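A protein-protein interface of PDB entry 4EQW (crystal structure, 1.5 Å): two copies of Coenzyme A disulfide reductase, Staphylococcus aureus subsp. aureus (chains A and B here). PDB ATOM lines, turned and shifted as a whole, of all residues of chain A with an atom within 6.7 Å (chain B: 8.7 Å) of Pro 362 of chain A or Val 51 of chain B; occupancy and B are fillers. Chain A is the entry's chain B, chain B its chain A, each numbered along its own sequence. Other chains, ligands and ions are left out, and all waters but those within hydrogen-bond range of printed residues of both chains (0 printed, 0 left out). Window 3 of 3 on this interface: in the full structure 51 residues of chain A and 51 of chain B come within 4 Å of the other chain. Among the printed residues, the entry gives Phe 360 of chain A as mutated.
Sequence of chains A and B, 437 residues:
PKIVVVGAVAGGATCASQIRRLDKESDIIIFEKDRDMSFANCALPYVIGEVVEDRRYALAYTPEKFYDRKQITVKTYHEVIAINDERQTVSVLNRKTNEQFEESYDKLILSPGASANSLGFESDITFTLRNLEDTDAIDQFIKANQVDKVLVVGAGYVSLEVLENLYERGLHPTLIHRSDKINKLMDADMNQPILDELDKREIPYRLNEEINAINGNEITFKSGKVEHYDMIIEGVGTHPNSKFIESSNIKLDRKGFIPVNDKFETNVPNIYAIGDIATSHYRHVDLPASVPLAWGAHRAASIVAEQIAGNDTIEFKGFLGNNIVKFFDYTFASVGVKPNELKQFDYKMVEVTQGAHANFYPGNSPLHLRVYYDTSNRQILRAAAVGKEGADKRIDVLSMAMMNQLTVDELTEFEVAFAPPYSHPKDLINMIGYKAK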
ATOM      1  N   HIS A 357       2.530  13.401   5.344  1.00  0.00           N
ATOM      2  CA  HIS A 357       2.053  13.829   4.038  1.00  0.00           C
ATOM      3  C   HIS A 357       2.297  12.724   3.030  1.00  0.00           C
ATOM      4  O   HIS A 357       2.642  11.608   3.411  1.00  0.00           O
ATOM      5  CB  HIS A 357       2.753  15.116   3.607  1.00  0.00           C
ATOM      6  CG  HIS A 357       4.244  15.001   3.537  1.00  0.00           C
ATOM      7  ND1 HIS A 357       5.087  15.750   4.332  1.00  0.00           N
ATOM      8  CD2 HIS A 357       5.044  14.223   2.771  1.00  0.00           C
ATOM      9  CE1 HIS A 357       6.340  15.441   4.055  1.00  0.00           C
ATOM     10  NE2 HIS A 357       6.342  14.515   3.111  1.00  0.00           N
ATOM     11  N   ALA A 358       2.118  13.043   1.750  1.00  0.00           N
ATOM     12  CA  ALA A 358       2.231  12.056   0.678  1.00  0.00           C
ATOM     13  C   ALA A 358       3.454  11.166   0.846  1.00  0.00           C
ATOM     14  O   ALA A 358       4.577  11.656   0.928  1.00  0.00           O
ATOM     15  CB  ALA A 358       2.269  12.747  -0.677  1.00  0.00           C
ATOM     16  N   ASN A 359       3.222   9.857   0.892  1.00  0.00           N
ATOM     17  CA  ASN A 359       4.298   8.891   1.073  1.00  0.00           C
ATOM     18  C   ASN A 359       5.388   9.060   0.026  1.00  0.00           C
ATOM     19  O   ASN A 359       6.577   8.990   0.336  1.00  0.00           O
ATOM     20  CB  ASN A 359       3.744   7.463   1.054  1.00  0.00           C
ATOM     21  CG  ASN A 359       2.861   7.167   2.256  1.00  0.00           C
ATOM     22  OD1 ASN A 359       3.213   7.491   3.392  1.00  0.00           O
ATOM     23  ND2 ASN A 359       1.709   6.550   2.009  1.00  0.00           N
ATOM     24  N   PHE A 360       4.976   9.297  -1.216  1.00  0.00           N
ATOM     25  CA  PHE A 360       5.924   9.508  -2.304  1.00  0.00           C
ATOM     26  C   PHE A 360       6.633  10.853  -2.187  1.00  0.00           C
ATOM     27  O   PHE A 360       7.641  11.092  -2.847  1.00  0.00           O
ATOM     28  CB  PHE A 360       5.220   9.404  -3.664  1.00  0.00           C
ATOM     29  CG  PHE A 360       4.166  10.453  -3.886  1.00  0.00           C
ATOM     30  CD1 PHE A 360       4.520  11.763  -4.173  1.00  0.00           C
ATOM     31  CD2 PHE A 360       2.821  10.126  -3.818  1.00  0.00           C
ATOM     32  CE1 PHE A 360       3.552  12.730  -4.381  1.00  0.00           C
ATOM     33  CE2 PHE A 360       1.846  11.089  -4.020  1.00  0.00           C
ATOM     34  CZ  PHE A 360       2.212  12.392  -4.302  1.00  0.00           C
ATOM     35  N   TYR A 361       6.099  11.732  -1.344  1.00  0.00           N
ATOM     36  CA  TYR A 361       6.614  13.093  -1.231  1.00  0.00           C
ATOM     37  C   TYR A 361       7.717  13.211  -0.180  1.00  0.00           C
ATOM     38  O   TYR A 361       7.563  12.747   0.950  1.00  0.00           O
ATOM     39  CB  TYR A 361       5.471  14.066  -0.922  1.00  0.00           C
ATOM     40  CG  TYR A 361       5.862  15.523  -1.003  1.00  0.00           C
ATOM     41  CD1 TYR A 361       5.729  16.234  -2.189  1.00  0.00           C
ATOM     42  CD2 TYR A 361       6.360  16.188   0.109  1.00  0.00           C
ATOM     43  CE1 TYR A 361       6.085  17.568  -2.264  1.00  0.00           C
ATOM     44  CE2 TYR A 361       6.713  17.523   0.043  1.00  0.00           C
ATOM     45  CZ  TYR A 361       6.576  18.206  -1.150  1.00  0.00           C
ATOM     46  OH  TYR A 361       6.931  19.532  -1.221  1.00  0.00           O
ATOM     47  N   PRO A 362       8.836  13.847  -0.560  1.00  0.00           N
ATOM     48  CA  PRO A 362      10.069  13.989   0.225  1.00  0.00           C
ATOM     49  C   PRO A 362       9.869  14.620   1.600  1.00  0.00           C
ATOM     50  O   PRO A 362       8.831  15.224   1.867  1.00  0.00           O
ATOM     51  CB  PRO A 362      10.925  14.920  -0.639  1.00  0.00           C
ATOM     52  CG  PRO A 362      10.432  14.707  -2.016  1.00  0.00           C
ATOM     53  CD  PRO A 362       8.958  14.473  -1.886  1.00  0.00           C
ATOM     54  N   GLY A 363      10.876  14.480   2.456  1.00  0.00           N
ATOM     55  CA  GLY A 363      10.847  15.067   3.782  1.00  0.00           C
ATOM     56  C   GLY A 363       9.757  14.487   4.659  1.00  0.00           C
ATOM     57  O   GLY A 363       9.368  15.096   5.653  1.00  0.00           O
ATOM     58  N   ASN A 364       9.265  13.308   4.295  1.00  0.00           N
ATOM     59  CA  ASN A 364       8.182  12.676   5.042  1.00  0.00           C
ATOM     60  C   ASN A 364       8.683  12.055   6.341  1.00  0.00           C
ATOM     61  O   ASN A 364       9.848  11.669   6.450  1.00  0.00           O
ATOM     62  CB  ASN A 364       7.464  11.629   4.185  1.00  0.00           C
ATOM     63  CG  ASN A 364       6.006  11.432   4.589  1.00  0.00           C
ATOM     64  OD1 ASN A 364       5.431  12.239   5.332  1.00  0.00           O
ATOM     65  ND2 ASN A 364       5.398  10.360   4.090  1.00  0.00           N
ATOM     66  N   SER A 365       7.792  11.969   7.323  1.00  0.00           N
ATOM     67  CA  SER A 365       8.115  11.397   8.620  1.00  0.00           C
ATOM     68  C   SER A 365       6.862  10.768   9.209  1.00  0.00           C
ATOM     69  O   SER A 365       5.768  11.306   9.067  1.00  0.00           O
ATOM     70  CB  SER A 365       8.647  12.477   9.561  1.00  0.00           C
ATOM     71  OG  SER A 365       7.729  13.555   9.672  1.00  0.00           O
ATOM     72  N   GLU A 389       6.454  15.800  12.055  1.00  0.00           N
ATOM     73  CA  GLU A 389       5.600  16.685  11.268  1.00  0.00           C
ATOM     74  C   GLU A 389       4.098  16.413  11.437  1.00  0.00           C
ATOM     75  O   GLU A 389       3.660  15.264  11.488  1.00  0.00           O
ATOM     76  CB  GLU A 389       5.980  16.581   9.787  1.00  0.00           C
ATOM     77  CG  GLU A 389       4.996  17.248   8.844  1.00  0.00           C
ATOM     78  CD  GLU A 389       5.482  17.254   7.407  1.00  0.00           C
ATOM     79  OE1 GLU A 389       4.630  17.315   6.494  1.00  0.00           O
ATOM     80  OE2 GLU A 389       6.713  17.194   7.191  1.00  0.00           O
ATOM     81  N   PRO A 421       2.258  17.924  -0.165  1.00  0.00           N
ATOM     82  CA  PRO A 421       3.082  18.358   0.971  1.00  0.00           C
ATOM     83  C   PRO A 421       2.355  18.341   2.314  1.00  0.00           C
ATOM     84  O   PRO A 421       3.019  18.535   3.340  1.00  0.00           O
ATOM     85  CB  PRO A 421       3.431  19.810   0.611  1.00  0.00           C
ATOM     86  CG  PRO A 421       3.227  19.899  -0.881  1.00  0.00           C
ATOM     87  CD  PRO A 421       2.046  19.016  -1.127  1.00  0.00           C
ATOM     88  N   ALA B  43       0.973  13.057  -7.732  1.00  0.00           N
ATOM     89  CA  ALA B  43       2.426  12.956  -7.776  1.00  0.00           C
ATOM     90  C   ALA B  43       3.005  13.384  -9.119  1.00  0.00           C
ATOM     91  O   ALA B  43       4.206  13.660  -9.230  1.00  0.00           O
ATOM     92  CB  ALA B  43       2.868  11.529  -7.444  1.00  0.00           C
ATOM     93  N   LEU B  44       2.162  13.439 -10.141  1.00  0.00           N
ATOM     94  CA  LEU B  44       2.673  13.609 -11.502  1.00  0.00           C
ATOM     95  C   LEU B  44       3.560  14.851 -11.710  1.00  0.00           C
ATOM     96  O   LEU B  44       4.603  14.760 -12.359  1.00  0.00           O
ATOM     97  CB  LEU B  44       1.534  13.530 -12.529  1.00  0.00           C
ATOM     98  CG  LEU B  44       0.747  12.211 -12.470  1.00  0.00           C
ATOM     99  CD1 LEU B  44      -0.384  12.213 -13.487  1.00  0.00           C
ATOM    100  CD2 LEU B  44       1.652  10.983 -12.672  1.00  0.00           C
ATOM    101  N   PRO B  45       3.172  16.011 -11.145  1.00  0.00           N
ATOM    102  CA  PRO B  45       4.051  17.172 -11.341  1.00  0.00           C
ATOM    103  C   PRO B  45       5.431  16.939 -10.736  1.00  0.00           C
ATOM    104  O   PRO B  45       6.438  17.436 -11.241  1.00  0.00           O
ATOM    105  CB  PRO B  45       3.321  18.290 -10.579  1.00  0.00           C
ATOM    106  CG  PRO B  45       1.876  17.871 -10.613  1.00  0.00           C
ATOM    107  CD  PRO B  45       1.911  16.376 -10.473  1.00  0.00           C
ATOM    108  N   TYR B  46       5.467  16.183  -9.648  1.00  0.00           N
ATOM    109  CA  TYR B  46       6.710  15.948  -8.933  1.00  0.00           C
ATOM    110  C   TYR B  46       7.567  14.896  -9.624  1.00  0.00           C
ATOM    111  O   TYR B  46       8.791  14.897  -9.492  1.00  0.00           O
ATOM    112  CB  TYR B  46       6.416  15.592  -7.474  1.00  0.00           C
ATOM    113  CG  TYR B  46       5.599  16.672  -6.801  1.00  0.00           C
ATOM    114  CD1 TYR B  46       4.215  16.581  -6.727  1.00  0.00           C
ATOM    115  CD2 TYR B  46       6.211  17.804  -6.279  1.00  0.00           C
ATOM    116  CE1 TYR B  46       3.466  17.576  -6.132  1.00  0.00           C
ATOM    117  CE2 TYR B  46       5.470  18.807  -5.688  1.00  0.00           C
ATOM    118  CZ  TYR B  46       4.101  18.686  -5.609  1.00  0.00           C
ATOM    119  OH  TYR B  46       3.372  19.687  -5.016  1.00  0.00           O
ATOM    120  N   VAL B  47       6.926  14.007 -10.377  1.00  0.00           N
ATOM    121  CA  VAL B  47       7.663  13.086 -11.229  1.00  0.00           C
ATOM    122  C   VAL B  47       8.373  13.886 -12.317  1.00  0.00           C
ATOM    123  O   VAL B  47       9.548  13.655 -12.608  1.00  0.00           O
ATOM    124  CB  VAL B  47       6.738  12.043 -11.873  1.00  0.00           C
ATOM    125  CG1 VAL B  47       7.506  11.217 -12.899  1.00  0.00           C
ATOM    126  CG2 VAL B  47       6.127  11.151 -10.799  1.00  0.00           C
ATOM    127  N   ILE B  48       7.661  14.843 -12.905  1.00  0.00           N
ATOM    128  CA  ILE B  48       8.249  15.719 -13.912  1.00  0.00           C
ATOM    129  C   ILE B  48       9.437  16.496 -13.334  1.00  0.00           C
ATOM    130  O   ILE B  48      10.447  16.705 -14.011  1.00  0.00           O
ATOM    131  CB  ILE B  48       7.191  16.690 -14.491  1.00  0.00           C
ATOM    132  CG1 ILE B  48       6.120  15.907 -15.260  1.00  0.00           C
ATOM    133  CG2 ILE B  48       7.847  17.754 -15.369  1.00  0.00           C
ATOM    134  CD1 ILE B  48       4.993  16.762 -15.794  1.00  0.00           C
ATOM    135  N   GLY B  49       9.319  16.902 -12.072  1.00  0.00           N
ATOM    136  CA  GLY B  49      10.366  17.673 -11.417  1.00  0.00           C
ATOM    137  C   GLY B  49      11.532  16.827 -10.935  1.00  0.00           C
ATOM    138  O   GLY B  49      12.514  17.352 -10.405  1.00  0.00           O
ATOM    139  N   GLU B  50      11.420  15.514 -11.114  1.00  0.00           N
ATOM    140  CA  GLU B  50      12.443  14.580 -10.652  1.00  0.00           C
ATOM    141  C   GLU B  50      12.607  14.650  -9.138  1.00  0.00           C
ATOM    142  O   GLU B  50      13.622  14.224  -8.587  1.00  0.00           O
ATOM    143  CB  GLU B  50      13.767  14.828 -11.376  1.00  0.00           C
ATOM    144  CG  GLU B  50      13.669  14.609 -12.878  1.00  0.00           C
ATOM    145  CD  GLU B  50      14.946  14.961 -13.621  1.00  0.00           C
ATOM    146  OE1 GLU B  50      15.102  14.513 -14.775  1.00  0.00           O
ATOM    147  OE2 GLU B  50      15.793  15.685 -13.054  1.00  0.00           O
ATOM    148  N   VAL B  51      11.593  15.205  -8.483  1.00  0.00           N
ATOM    149  CA  VAL B  51      11.474  15.192  -7.033  1.00  0.00           C
ATOM    150  C   VAL B  51      11.063  13.785  -6.630  1.00  0.00           C
ATOM    151  O   VAL B  51      11.506  13.252  -5.612  1.00  0.00           O
ATOM    152  CB  VAL B  51      10.408  16.196  -6.560  1.00  0.00           C
ATOM    153  CG1 VAL B  51       9.922  15.852  -5.166  1.00  0.00           C
ATOM    154  CG2 VAL B  51      10.952  17.617  -6.609  1.00  0.00           C
ATOM    155  N   VAL B  52      10.203  13.189  -7.449  1.00  0.00           N
ATOM    156  CA  VAL B  52       9.873  11.780  -7.322  1.00  0.00           C
ATOM    157  C   VAL B  52      10.658  11.011  -8.379  1.00  0.00           C
ATOM    158  O   VAL B  52      10.301  11.000  -9.560  1.00  0.00           O
ATOM    159  CB  VAL B  52       8.361  11.521  -7.489  1.00  0.00           C
ATOM    160  CG1 VAL B  52       8.089  10.028  -7.579  1.00  0.00           C
ATOM    161  CG2 VAL B  52       7.587  12.132  -6.336  1.00  0.00           C
ATOM    162  N   GLU B  53      11.747  10.388  -7.946  1.00  0.00           N
ATOM    163  CA  GLU B  53      12.624   9.646  -8.840  1.00  0.00           C
ATOM    164  C   GLU B  53      12.115   8.222  -9.006  1.00  0.00           C
ATOM    165  O   GLU B  53      12.022   7.704 -10.119  1.00  0.00           O
ATOM    166  CB  GLU B  53      14.043   9.608  -8.266  1.00  0.00           C
ATOM    167  CG  GLU B  53      14.667  10.974  -8.006  1.00  0.00           C
ATOM    168  CD  GLU B  53      15.413  11.509  -9.214  1.00  0.00           C
ATOM    169  OE1 GLU B  53      16.393  12.264  -9.025  1.00  0.00           O
ATOM    170  OE2 GLU B  53      15.025  11.165 -10.350  1.00  0.00           O
ATOM    171  N   ASP B  54      11.789   7.599  -7.878  1.00  0.00           N
ATOM    172  CA  ASP B  54      11.355   6.209  -7.840  1.00  0.00           C
ATOM    173  C   ASP B  54       9.960   6.057  -8.440  1.00  0.00           C
ATOM    174  O   ASP B  54       8.962   6.305  -7.768  1.00  0.00           O
ATOM    175  CB  ASP B  54      11.358   5.718  -6.389  1.00  0.00           C
ATOM    176  CG  ASP B  54      11.254   4.208  -6.278  1.00  0.00           C
ATOM    177  OD1 ASP B  54      11.437   3.684  -5.157  1.00  0.00           O
ATOM    178  OD2 ASP B  54      10.994   3.545  -7.303  1.00  0.00           O
ATOM    179  N   TYR B  57       6.800   5.092  -6.869  1.00  0.00           N
ATOM    180  CA  TYR B  57       5.995   6.039  -6.105  1.00  0.00           C
ATOM    181  C   TYR B  57       4.809   6.551  -6.918  1.00  0.00           C
ATOM    182  O   TYR B  57       3.845   7.078  -6.365  1.00  0.00           O
ATOM    183  CB  TYR B  57       6.849   7.235  -5.679  1.00  0.00           C
ATOM    184  CG  TYR B  57       7.549   7.086  -4.345  1.00  0.00           C
ATOM    185  CD1 TYR B  57       8.868   7.489  -4.186  1.00  0.00           C
ATOM    186  CD2 TYR B  57       6.889   6.551  -3.245  1.00  0.00           C
ATOM    187  CE1 TYR B  57       9.513   7.366  -2.967  1.00  0.00           C
ATOM    188  CE2 TYR B  57       7.525   6.423  -2.021  1.00  0.00           C
ATOM    189  CZ  TYR B  57       8.838   6.831  -1.888  1.00  0.00           C
ATOM    190  OH  TYR B  57       9.482   6.705  -0.676  1.00  0.00           O
ATOM    191  N   GLU B 161       2.129  23.940  -9.916  1.00  0.00           N
ATOM    192  CA  GLU B 161       2.984  22.864  -9.428  1.00  0.00           C
ATOM    193  C   GLU B 161       3.905  22.371 -10.543  1.00  0.00           C
ATOM    194  O   GLU B 161       5.074  22.067 -10.312  1.00  0.00           O
ATOM    195  CB  GLU B 161       2.149  21.701  -8.895  1.00  0.00           C
ATOM    196  CG  GLU B 161       1.380  21.999  -7.620  1.00  0.00           C
ATOM    197  CD  GLU B 161       0.617  20.785  -7.128  1.00  0.00           C
ATOM    198  OE1 GLU B 161       0.676  19.745  -7.811  1.00  0.00           O
ATOM    199  OE2 GLU B 161      -0.040  20.865  -6.065  1.00  0.00           O
ATOM    200  N   GLU B 164       6.752  25.021 -10.954  1.00  0.00           N
ATOM    201  CA  GLU B 164       7.766  24.925  -9.912  1.00  0.00           C
ATOM    202  C   GLU B 164       8.697  23.740 -10.155  1.00  0.00           C
ATOM    203  O   GLU B 164       9.921  23.863 -10.053  1.00  0.00           O
ATOM    204  CB  GLU B 164       7.143  24.841  -8.516  1.00  0.00           C
ATOM    205  CG  GLU B 164       8.166  24.513  -7.435  1.00  0.00           C
ATOM    206  CD  GLU B 164       7.651  24.764  -6.035  1.00  0.00           C
ATOM    207  OE1 GLU B 164       6.440  25.016  -5.873  1.00  0.00           O
ATOM    208  OE2 GLU B 164       8.468  24.702  -5.091  1.00  0.00           O
ATOM    209  N   ASN B 165       8.113  22.592 -10.482  1.00  0.00           N
ATOM    210  CA  ASN B 165       8.895  21.393 -10.761  1.00  0.00           C
ATOM    211  C   ASN B 165       9.831  21.501 -11.960  1.00  0.00           C
ATOM    212  O   ASN B 165      10.962  21.027 -11.903  1.00  0.00           O
ATOM    213  CB  ASN B 165       7.981  20.177 -10.886  1.00  0.00           C
ATOM    214  CG  ASN B 165       7.623  19.603  -9.540  1.00  0.00           C
ATOM    215  OD1 ASN B 165       8.417  18.884  -8.937  1.00  0.00           O
ATOM    216  ND2 ASN B 165       6.439  19.948  -9.041  1.00  0.00           N
ATOM    217  N   LEU B 166       9.363  22.127 -13.035  1.00  0.00           N
ATOM    218  CA  LEU B 166      10.220  22.395 -14.190  1.00  0.00           C
ATOM    219  C   LEU B 166      11.395  23.287 -13.794  1.00  0.00           C
ATOM    220  O   LEU B 166      12.538  23.042 -14.189  1.00  0.00           O
ATOM    221  CB  LEU B 166       9.421  23.045 -15.323  1.00  0.00           C
ATOM    222  CG  LEU B 166       8.377  22.169 -16.015  1.00  0.00           C
ATOM    223  CD1 LEU B 166       7.507  23.026 -16.931  1.00  0.00           C
ATOM    224  CD2 LEU B 166       9.051  21.053 -16.796  1.00  0.00           C
ATOM    225  N   GLU B 168      12.730  23.668 -10.747  1.00  0.00           N
ATOM    226  CA  GLU B 168      13.662  22.967  -9.867  1.00  0.00           C
ATOM    227  C   GLU B 168      14.466  21.897 -10.619  1.00  0.00           C
ATOM    228  O   GLU B 168      15.589  21.568 -10.228  1.00  0.00           O
ATOM    229  CB  GLU B 168      12.940  22.365  -8.659  1.00  0.00           C
ATOM    230  CG  GLU B 168      12.318  23.401  -7.723  1.00  0.00           C
ATOM    231  CD  GLU B 168      13.341  24.334  -7.079  1.00  0.00           C
ATOM    232  OE1 GLU B 168      12.929  25.369  -6.512  1.00  0.00           O
ATOM    233  OE2 GLU B 168      14.556  24.036  -7.141  1.00  0.00           O
ATOM    234  N   ARG B 169      13.892  21.366 -11.696  1.00  0.00           N
ATOM    235  CA  ARG B 169      14.586  20.385 -12.527  1.00  0.00           C
ATOM    236  C   ARG B 169      15.715  21.047 -13.315  1.00  0.00           C
ATOM    237  O   ARG B 169      16.588  20.366 -13.867  1.00  0.00           O
ATOM    238  CB  ARG B 169      13.598  19.690 -13.473  1.00  0.00           C
ATOM    239  CG  ARG B 169      14.225  18.677 -14.433  1.00  0.00           C
ATOM    240  CD  ARG B 169      13.156  17.834 -15.108  1.00  0.00           C
ATOM    241  NE  ARG B 169      13.692  17.014 -16.193  1.00  0.00           N
ATOM    242  CZ  ARG B 169      13.072  15.954 -16.701  1.00  0.00           C
ATOM    243  NH1 ARG B 169      11.900  15.568 -16.213  1.00  0.00           N
ATOM    244  NH2 ARG B 169      13.630  15.266 -17.690  1.00  0.00           N
ATOM    245  N   LYS B 326       0.853  24.322  -2.530  1.00  0.00           N
ATOM    246  CA  LYS B 326       2.138  24.915  -2.190  1.00  0.00           C
ATOM    247  C   LYS B 326       2.712  25.504  -3.457  1.00  0.00           C
ATOM    248  O   LYS B 326       2.637  24.879  -4.519  1.00  0.00           O
ATOM    249  CB  LYS B 326       3.095  23.855  -1.638  1.00  0.00           C
ATOM    250  CG  LYS B 326       4.571  24.202  -1.820  1.00  0.00           C
ATOM    251  CD  LYS B 326       5.467  22.974  -1.660  1.00  0.00           C
ATOM    252  CE  LYS B 326       6.658  23.006  -2.626  1.00  0.00           C
ATOM    253  NZ  LYS B 326       7.506  24.237  -2.516  1.00  0.00           N
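Among the printed residues, merely in contact across the chains: Phe 360 of chain A with Tyr 57 of chain B (3.2 Å), Phe 360 of chain A with Ala 43 of chain B (3.3 Å), Pro 362 of chain A with Val 51 of chain B (3.4 Å), Asn 359 of chain A with Tyr 57 of chain B (3.6 Å), Phe 360 of chain A with Val 52 of chain B (3.6 Å), Tyr 361 of chain A with Tyr 46 of chain B (3.7 Å), Tyr 361 of chain A with Lys 326 of chain B (3.8 Å) and Pro 421 of chain A with Lys 326 of chain B (3.9 Å).
Of chain A, only Pro 362 (3.4 Å) comes within 4 Å of Val 51 of chain B. Of the printed residues of chain A, Tyr 46 of chain B touches Tyr 361 (3.7 Å). Of the printed residues of chain A, Lys 326 of chain B touches Tyr 361 (3.8 Å) and Pro 421 (3.9 Å). Printed residues of chain A within 4 Å of Ala 43 of chain B: Phe 360. Printed residues of chain A within 4 Å of Tyr 57 of chain B: Asn 359 and Phe 360. Printed residues of chain B within 4 Å of Pro 421 of chain A: Lys 326. Arg 169 of chain B touches none of the printed residues of chain A. Glu 161 of chain B touches none of the printed residues of chain A. The nearest residue of chain B that does not touch Pro 362 of chain A is Val 52 of chain B (5.2 Å). The nearest printed residue of chain B that does not touch Phe 360 of chain A is Tyr 46 of chain B (4.6 Å).
O of Pro 362 of chain A lies within hydrogen-bond range of NE2 of His 357 of chain A (2.9 Å). N of Val 51 of chain B sits at hydrogen-bond distance from O of Tyr 46 of chain B, 3.0 Å away. A ring nitrogen (NE2) of His 357 of chain A sits at hydrogen-bond distance from the backbone carbonyl oxygen of Tyr 361 of chain A. The backbone carbonyl oxygen (O) of Tyr 46 of chain B lies within hydrogen-bond range of the backbone NH (N) of Val 52 of chain B (3.0 Å). The side-chain carboxylate of Glu 164 of chain B lies within salt-bridge range of the side-chain amino group of Lys 326 of chain B (2.8 Å).
Of the 11 printed residues of chain A, 5 touch a printed residue of chain B. Among the printed residues, no Asp or Glu carboxylate lies within 4 Å of a Lys or Arg side-chain nitrogen of the other chain.
No position is printed for both chains.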
